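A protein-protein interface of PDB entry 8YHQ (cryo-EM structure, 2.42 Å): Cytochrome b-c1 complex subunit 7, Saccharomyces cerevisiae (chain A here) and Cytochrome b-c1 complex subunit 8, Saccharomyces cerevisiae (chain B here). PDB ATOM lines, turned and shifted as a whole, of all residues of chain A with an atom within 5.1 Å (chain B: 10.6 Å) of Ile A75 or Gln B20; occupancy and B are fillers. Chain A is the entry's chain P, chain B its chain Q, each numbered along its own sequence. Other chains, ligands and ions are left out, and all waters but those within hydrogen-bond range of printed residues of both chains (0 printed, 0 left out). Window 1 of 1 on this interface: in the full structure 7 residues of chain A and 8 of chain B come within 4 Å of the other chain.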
ATOM      1  N   TYR A  68      -8.952   7.604  12.914  1.00  0.00           N
ATOM      2  CA  TYR A  68      -9.274   7.167  11.562  1.00  0.00           C
ATOM      3  C   TYR A  68      -8.017   7.087  10.709  1.00  0.00           C
ATOM      4  O   TYR A  68      -7.886   6.192   9.870  1.00  0.00           O
ATOM      5  CB  TYR A  68     -10.294   8.116  10.921  1.00  0.00           C
ATOM      6  CG  TYR A  68     -11.685   8.108  11.505  1.00  0.00           C
ATOM      7  CD1 TYR A  68     -12.337   6.927  11.803  1.00  0.00           C
ATOM      8  CD2 TYR A  68     -12.358   9.293  11.729  1.00  0.00           C
ATOM      9  CE1 TYR A  68     -13.599   6.928  12.324  1.00  0.00           C
ATOM     10  CE2 TYR A  68     -13.620   9.299  12.248  1.00  0.00           C
ATOM     11  CZ  TYR A  68     -14.236   8.116  12.543  1.00  0.00           C
ATOM     12  OH  TYR A  68     -15.499   8.130  13.063  1.00  0.00           O
ATOM     13  N   ALA A  71      -5.921   3.848  11.418  1.00  0.00           N
ATOM     14  CA  ALA A  71      -6.456   2.657  10.768  1.00  0.00           C
ATOM     15  C   ALA A  71      -6.047   2.580   9.302  1.00  0.00           C
ATOM     16  O   ALA A  71      -5.842   1.486   8.768  1.00  0.00           O
ATOM     17  CB  ALA A  71      -7.975   2.628  10.896  1.00  0.00           C
ATOM     18  N   TYR A  72      -5.932   3.724   8.632  1.00  0.00           N
ATOM     19  CA  TYR A  72      -5.586   3.718   7.217  1.00  0.00           C
ATOM     20  C   TYR A  72      -4.109   3.411   7.008  1.00  0.00           C
ATOM     21  O   TYR A  72      -3.743   2.688   6.075  1.00  0.00           O
ATOM     22  CB  TYR A  72      -5.950   5.056   6.581  1.00  0.00           C
ATOM     23  CG  TYR A  72      -5.415   5.218   5.188  1.00  0.00           C
ATOM     24  CD1 TYR A  72      -5.829   4.386   4.163  1.00  0.00           C
ATOM     25  CD2 TYR A  72      -4.485   6.193   4.899  1.00  0.00           C
ATOM     26  CE1 TYR A  72      -5.339   4.525   2.907  1.00  0.00           C
ATOM     27  CE2 TYR A  72      -3.990   6.340   3.641  1.00  0.00           C
ATOM     28  CZ  TYR A  72      -4.418   5.505   2.644  1.00  0.00           C
ATOM     29  OH  TYR A  72      -3.917   5.657   1.383  1.00  0.00           O
ATOM     30  N   ARG A  73      -3.243   3.965   7.857  1.00  0.00           N
ATOM     31  CA  ARG A  73      -1.817   3.686   7.755  1.00  0.00           C
ATOM     32  C   ARG A  73      -1.524   2.207   7.961  1.00  0.00           C
ATOM     33  O   ARG A  73      -0.590   1.664   7.363  1.00  0.00           O
ATOM     34  CB  ARG A  73      -1.050   4.527   8.769  1.00  0.00           C
ATOM     35  CG  ARG A  73      -0.997   5.992   8.441  1.00  0.00           C
ATOM     36  CD  ARG A  73       0.010   6.739   9.292  1.00  0.00           C
ATOM     37  NE  ARG A  73      -0.290   6.651  10.713  1.00  0.00           N
ATOM     38  CZ  ARG A  73      -0.979   7.544  11.420  1.00  0.00           C
ATOM     39  NH1 ARG A  73      -1.174   7.319  12.703  1.00  0.00           N
ATOM     40  NH2 ARG A  73      -1.468   8.652  10.881  1.00  0.00           N
ATOM     41  N   ILE A  74      -2.318   1.537   8.796  1.00  0.00           N
ATOM     42  CA  ILE A  74      -2.074   0.137   9.106  1.00  0.00           C
ATOM     43  C   ILE A  74      -2.548  -0.758   7.967  1.00  0.00           C
ATOM     44  O   ILE A  74      -1.906  -1.763   7.646  1.00  0.00           O
ATOM     45  CB  ILE A  74      -2.730  -0.213  10.458  1.00  0.00           C
ATOM     46  CG1 ILE A  74      -1.798   0.213  11.599  1.00  0.00           C
ATOM     47  CG2 ILE A  74      -3.078  -1.690  10.581  1.00  0.00           C
ATOM     48  CD1 ILE A  74      -2.439   0.315  12.956  1.00  0.00           C
ATOM     49  N   ILE A  75      -3.672  -0.414   7.341  1.00  0.00           N
ATOM     50  CA  ILE A  75      -4.163  -1.167   6.192  1.00  0.00           C
ATOM     51  C   ILE A  75      -3.234  -0.990   4.998  1.00  0.00           C
ATOM     52  O   ILE A  75      -2.926  -1.952   4.288  1.00  0.00           O
ATOM     53  CB  ILE A  75      -5.607  -0.740   5.883  1.00  0.00           C
ATOM     54  CG1 ILE A  75      -6.551  -1.402   6.882  1.00  0.00           C
ATOM     55  CG2 ILE A  75      -6.011  -1.075   4.457  1.00  0.00           C
ATOM     56  CD1 ILE A  75      -7.934  -0.828   6.921  1.00  0.00           C
ATOM     57  N   ARG A  76      -2.787   0.238   4.750  1.00  0.00           N
ATOM     58  CA  ARG A  76      -1.868   0.508   3.653  1.00  0.00           C
ATOM     59  C   ARG A  76      -0.554  -0.258   3.800  1.00  0.00           C
ATOM     60  O   ARG A  76       0.046  -0.667   2.801  1.00  0.00           O
ATOM     61  CB  ARG A  76      -1.630   2.014   3.567  1.00  0.00           C
ATOM     62  CG  ARG A  76      -0.738   2.482   2.451  1.00  0.00           C
ATOM     63  CD  ARG A  76      -0.645   3.987   2.404  1.00  0.00           C
ATOM     64  NE  ARG A  76       0.039   4.554   3.556  1.00  0.00           N
ATOM     65  CZ  ARG A  76       0.442   5.816   3.651  1.00  0.00           C
ATOM     66  NH1 ARG A  76       1.051   6.224   4.745  1.00  0.00           N
ATOM     67  NH2 ARG A  76       0.247   6.676   2.668  1.00  0.00           N
ATOM     68  N   ALA A  77      -0.087  -0.461   5.034  1.00  0.00           N
ATOM     69  CA  ALA A  77       1.185  -1.143   5.246  1.00  0.00           C
ATOM     70  C   ALA A  77       1.063  -2.650   5.051  1.00  0.00           C
ATOM     71  O   ALA A  77       1.996  -3.288   4.555  1.00  0.00           O
ATOM     72  CB  ALA A  77       1.726  -0.828   6.634  1.00  0.00           C
ATOM     73  N   HIS A  78      -0.057  -3.245   5.463  1.00  0.00           N
ATOM     74  CA  HIS A  78      -0.278  -4.661   5.201  1.00  0.00           C
ATOM     75  C   HIS A  78      -0.308  -4.948   3.704  1.00  0.00           C
ATOM     76  O   HIS A  78       0.244  -5.954   3.245  1.00  0.00           O
ATOM     77  CB  HIS A  78      -1.581  -5.128   5.848  1.00  0.00           C
ATOM     78  CG  HIS A  78      -1.488  -5.384   7.317  1.00  0.00           C
ATOM     79  ND1 HIS A  78      -0.431  -6.045   7.900  1.00  0.00           N
ATOM     80  CD2 HIS A  78      -2.342  -5.086   8.322  1.00  0.00           C
ATOM     81  CE1 HIS A  78      -0.631  -6.132   9.200  1.00  0.00           C
ATOM     82  NE2 HIS A  78      -1.781  -5.557   9.483  1.00  0.00           N
ATOM     83  N   GLN A  79      -0.962  -4.082   2.927  1.00  0.00           N
ATOM     84  CA  GLN A  79      -1.054  -4.278   1.487  1.00  0.00           C
ATOM     85  C   GLN A  79       0.298  -4.078   0.818  1.00  0.00           C
ATOM     86  O   GLN A  79       0.622  -4.763  -0.156  1.00  0.00           O
ATOM     87  CB  GLN A  79      -2.104  -3.325   0.908  1.00  0.00           C
ATOM     88  CG  GLN A  79      -2.421  -3.471  -0.566  1.00  0.00           C
ATOM     89  CD  GLN A  79      -3.213  -4.712  -0.890  1.00  0.00           C
ATOM     90  OE1 GLN A  79      -4.002  -5.191  -0.083  1.00  0.00           O
ATOM     91  NE2 GLN A  79      -3.009  -5.236  -2.080  1.00  0.00           N
ATOM     92  N   GLY B  13     -18.048  -9.584  11.061  1.00  0.00           N
ATOM     93  CA  GLY B  13     -19.030  -8.635  11.535  1.00  0.00           C
ATOM     94  C   GLY B  13     -18.646  -7.952  12.831  1.00  0.00           C
ATOM     95  O   GLY B  13     -19.001  -6.785  13.033  1.00  0.00           O
ATOM     96  N   MET B  15     -15.197  -8.272  14.344  1.00  0.00           N
ATOM     97  CA  MET B  15     -13.813  -8.725  14.444  1.00  0.00           C
ATOM     98  C   MET B  15     -13.065  -8.078  15.601  1.00  0.00           C
ATOM     99  O   MET B  15     -12.083  -8.645  16.091  1.00  0.00           O
ATOM    100  CB  MET B  15     -13.076  -8.452  13.135  1.00  0.00           C
ATOM    101  CG  MET B  15     -11.840  -9.310  12.906  1.00  0.00           C
ATOM    102  SD  MET B  15     -12.146 -11.080  12.757  1.00  0.00           S
ATOM    103  CE  MET B  15     -12.967 -11.156  11.176  1.00  0.00           C
ATOM    104  N   GLY B  16     -13.485  -6.899  16.034  1.00  0.00           N
ATOM    105  CA  GLY B  16     -12.939  -6.275  17.214  1.00  0.00           C
ATOM    106  C   GLY B  16     -11.840  -5.267  16.995  1.00  0.00           C
ATOM    107  O   GLY B  16     -10.974  -5.134  17.865  1.00  0.00           O
ATOM    108  N   GLY B  17     -11.840  -4.563  15.872  1.00  0.00           N
ATOM    109  CA  GLY B  17     -10.917  -3.485  15.634  1.00  0.00           C
ATOM    110  C   GLY B  17     -11.557  -2.129  15.830  1.00  0.00           C
ATOM    111  O   GLY B  17     -12.682  -2.012  16.326  1.00  0.00           O
ATOM    112  N   PRO B  18     -10.849  -1.072  15.449  1.00  0.00           N
ATOM    113  CA  PRO B  18     -11.428   0.267  15.535  1.00  0.00           C
ATOM    114  C   PRO B  18     -12.407   0.539  14.407  1.00  0.00           C
ATOM    115  O   PRO B  18     -12.368  -0.089  13.348  1.00  0.00           O
ATOM    116  CB  PRO B  18     -10.209   1.182  15.440  1.00  0.00           C
ATOM    117  CG  PRO B  18      -9.236   0.419  14.674  1.00  0.00           C
ATOM    118  CD  PRO B  18      -9.451  -1.027  15.000  1.00  0.00           C
ATOM    119  N   LYS B  19     -13.297   1.493  14.653  1.00  0.00           N
ATOM    120  CA  LYS B  19     -14.258   1.906  13.643  1.00  0.00           C
ATOM    121  C   LYS B  19     -13.557   2.645  12.512  1.00  0.00           C
ATOM    122  O   LYS B  19     -12.694   3.495  12.743  1.00  0.00           O
ATOM    123  CB  LYS B  19     -15.334   2.786  14.274  1.00  0.00           C
ATOM    124  CG  LYS B  19     -16.332   2.017  15.102  1.00  0.00           C
ATOM    125  CD  LYS B  19     -17.476   2.897  15.552  1.00  0.00           C
ATOM    126  CE  LYS B  19     -18.355   2.220  16.579  1.00  0.00           C
ATOM    127  NZ  LYS B  19     -18.556   0.779  16.323  1.00  0.00           N
ATOM    128  N   GLN B  20     -13.929   2.302  11.281  1.00  0.00           N
ATOM    129  CA  GLN B  20     -13.339   2.868  10.077  1.00  0.00           C
ATOM    130  C   GLN B  20     -14.334   3.792   9.391  1.00  0.00           C
ATOM    131  O   GLN B  20     -15.533   3.503   9.338  1.00  0.00           O
ATOM    132  CB  GLN B  20     -12.905   1.775   9.103  1.00  0.00           C
ATOM    133  CG  GLN B  20     -12.033   0.702   9.691  1.00  0.00           C
ATOM    134  CD  GLN B  20     -11.543  -0.282   8.655  1.00  0.00           C
ATOM    135  OE1 GLN B  20     -11.680  -0.062   7.456  1.00  0.00           O
ATOM    136  NE2 GLN B  20     -11.000  -1.392   9.114  1.00  0.00           N
ATOM    137  N   LYS B  21     -13.819   4.893   8.852  1.00  0.00           N
ATOM    138  CA  LYS B  21     -14.611   5.865   8.121  1.00  0.00           C
ATOM    139  C   LYS B  21     -13.685   6.581   7.155  1.00  0.00           C
ATOM    140  O   LYS B  21     -12.598   7.018   7.541  1.00  0.00           O
ATOM    141  CB  LYS B  21     -15.285   6.859   9.072  1.00  0.00           C
ATOM    142  CG  LYS B  21     -16.388   7.700   8.481  1.00  0.00           C
ATOM    143  CD  LYS B  21     -16.903   8.667   9.508  1.00  0.00           C
ATOM    144  CE  LYS B  21     -17.780   9.737   8.915  1.00  0.00           C
ATOM    145  NZ  LYS B  21     -19.072   9.216   8.433  1.00  0.00           N
ATOM    146  N   GLY B  22     -14.105   6.668   5.899  1.00  0.00           N
ATOM    147  CA  GLY B  22     -13.388   7.433   4.903  1.00  0.00           C
ATOM    148  C   GLY B  22     -12.388   6.676   4.063  1.00  0.00           C
ATOM    149  O   GLY B  22     -11.568   7.314   3.395  1.00  0.00           O
ATOM    150  N   ILE B  23     -12.434   5.344   4.056  1.00  0.00           N
ATOM    151  CA  ILE B  23     -11.533   4.513   3.262  1.00  0.00           C
ATOM    152  C   ILE B  23     -12.344   3.822   2.176  1.00  0.00           C
ATOM    153  O   ILE B  23     -13.408   3.257   2.451  1.00  0.00           O
ATOM    154  CB  ILE B  23     -10.783   3.479   4.123  1.00  0.00           C
ATOM    155  CG1 ILE B  23      -9.921   4.165   5.182  1.00  0.00           C
ATOM    156  CG2 ILE B  23      -9.892   2.620   3.241  1.00  0.00           C
ATOM    157  CD1 ILE B  23      -9.464   3.269   6.288  1.00  0.00           C
ATOM    158  N   THR B  24     -11.831   3.864   0.949  1.00  0.00           N
ATOM    159  CA  THR B  24     -12.447   3.234  -0.211  1.00  0.00           C
ATOM    160  C   THR B  24     -11.488   2.231  -0.843  1.00  0.00           C
ATOM    161  O   THR B  24     -10.292   2.496  -0.981  1.00  0.00           O
ATOM    162  CB  THR B  24     -12.856   4.291  -1.244  1.00  0.00           C
ATOM    163  OG1 THR B  24     -13.520   5.369  -0.585  1.00  0.00           O
ATOM    164  CG2 THR B  24     -13.785   3.712  -2.296  1.00  0.00           C
ATOM    165  N   SER B  25     -12.035   1.076  -1.230  1.00  0.00           N
ATOM    166  CA  SER B  25     -11.286  -0.022  -1.835  1.00  0.00           C
ATOM    167  C   SER B  25     -11.801  -0.311  -3.240  1.00  0.00           C
ATOM    168  O   SER B  25     -13.013  -0.318  -3.466  1.00  0.00           O
ATOM    169  CB  SER B  25     -11.389  -1.286  -0.977  1.00  0.00           C
ATOM    170  OG  SER B  25     -10.490  -2.281  -1.415  1.00  0.00           O
ATOM    171  N   TYR B  26     -10.877  -0.560  -4.173  1.00  0.00           N
ATOM    172  CA  TYR B  26     -11.187  -0.944  -5.546  1.00  0.00           C
ATOM    173  C   TYR B  26     -10.434  -2.216  -5.929  1.00  0.00           C
ATOM    174  O   TYR B  26      -9.332  -2.469  -5.440  1.00  0.00           O
ATOM    175  CB  TYR B  26     -10.814   0.152  -6.549  1.00  0.00           C
ATOM    176  CG  TYR B  26     -11.268   1.550  -6.231  1.00  0.00           C
ATOM    177  CD1 TYR B  26     -10.514   2.377  -5.418  1.00  0.00           C
ATOM    178  CD2 TYR B  26     -12.427   2.061  -6.784  1.00  0.00           C
ATOM    179  CE1 TYR B  26     -10.913   3.655  -5.146  1.00  0.00           C
ATOM    180  CE2 TYR B  26     -12.833   3.340  -6.516  1.00  0.00           C
ATOM    181  CZ  TYR B  26     -12.072   4.136  -5.697  1.00  0.00           C
ATOM    182  OH  TYR B  26     -12.477   5.415  -5.426  1.00  0.00           O
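No residue of chain B comes within 4 Å of Ala A71.
Of the printed residues of chain B, Tyr A72 touches Ile B23 (3.95 Å).
No residue of chain B comes within 4 Å of Ile A74.
Ile A75 touches one residue of chain B.
Gly B17 touches none of the printed residues of chain A.
Of the printed residues of chain A, Lys B19 touches Tyr A68.
Gln B20 touches just one residue of chain A: Ile A75.
Of the printed residues of chain A, Lys B21 touches Tyr A68 (3.7 Å).
Gly B22 touches none of the printed residues of chain A.
Of the printed residues of chain A, Ile B23 touches Tyr A72.
The nearest residue of chain A that does not touch Gln B20 is Tyr A68 (4.4 Å).
CE1 of Tyr A68 touches O of Lys B19, at 3.6 Å.
Tyr A68 touches Lys B21 (CE1 to CB, 3.7 Å).
CB of Tyr A72 touches CD1 of Ile B23 (3.95 Å).
Gln B20 touches Ile A75 (NE2 to CD1, 3.8 Å).
Of the 10 printed residues of chain A, 3 touch a printed residue of chain B.
Printed residues of chain A that touch a printed residue of chain B: Tyr A68, Tyr A72 and Ile A75.
Hydrophobic or aromatic side chains of chain A that line the printed part of chain B: Tyr A68, Tyr A72 and Ile A75.
Of the 13 printed residues of chain B, 4 touch a printed residue of chain A.
Hydrophobic or aromatic side chains of chain B that line the printed part of chain A: Ile B23.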
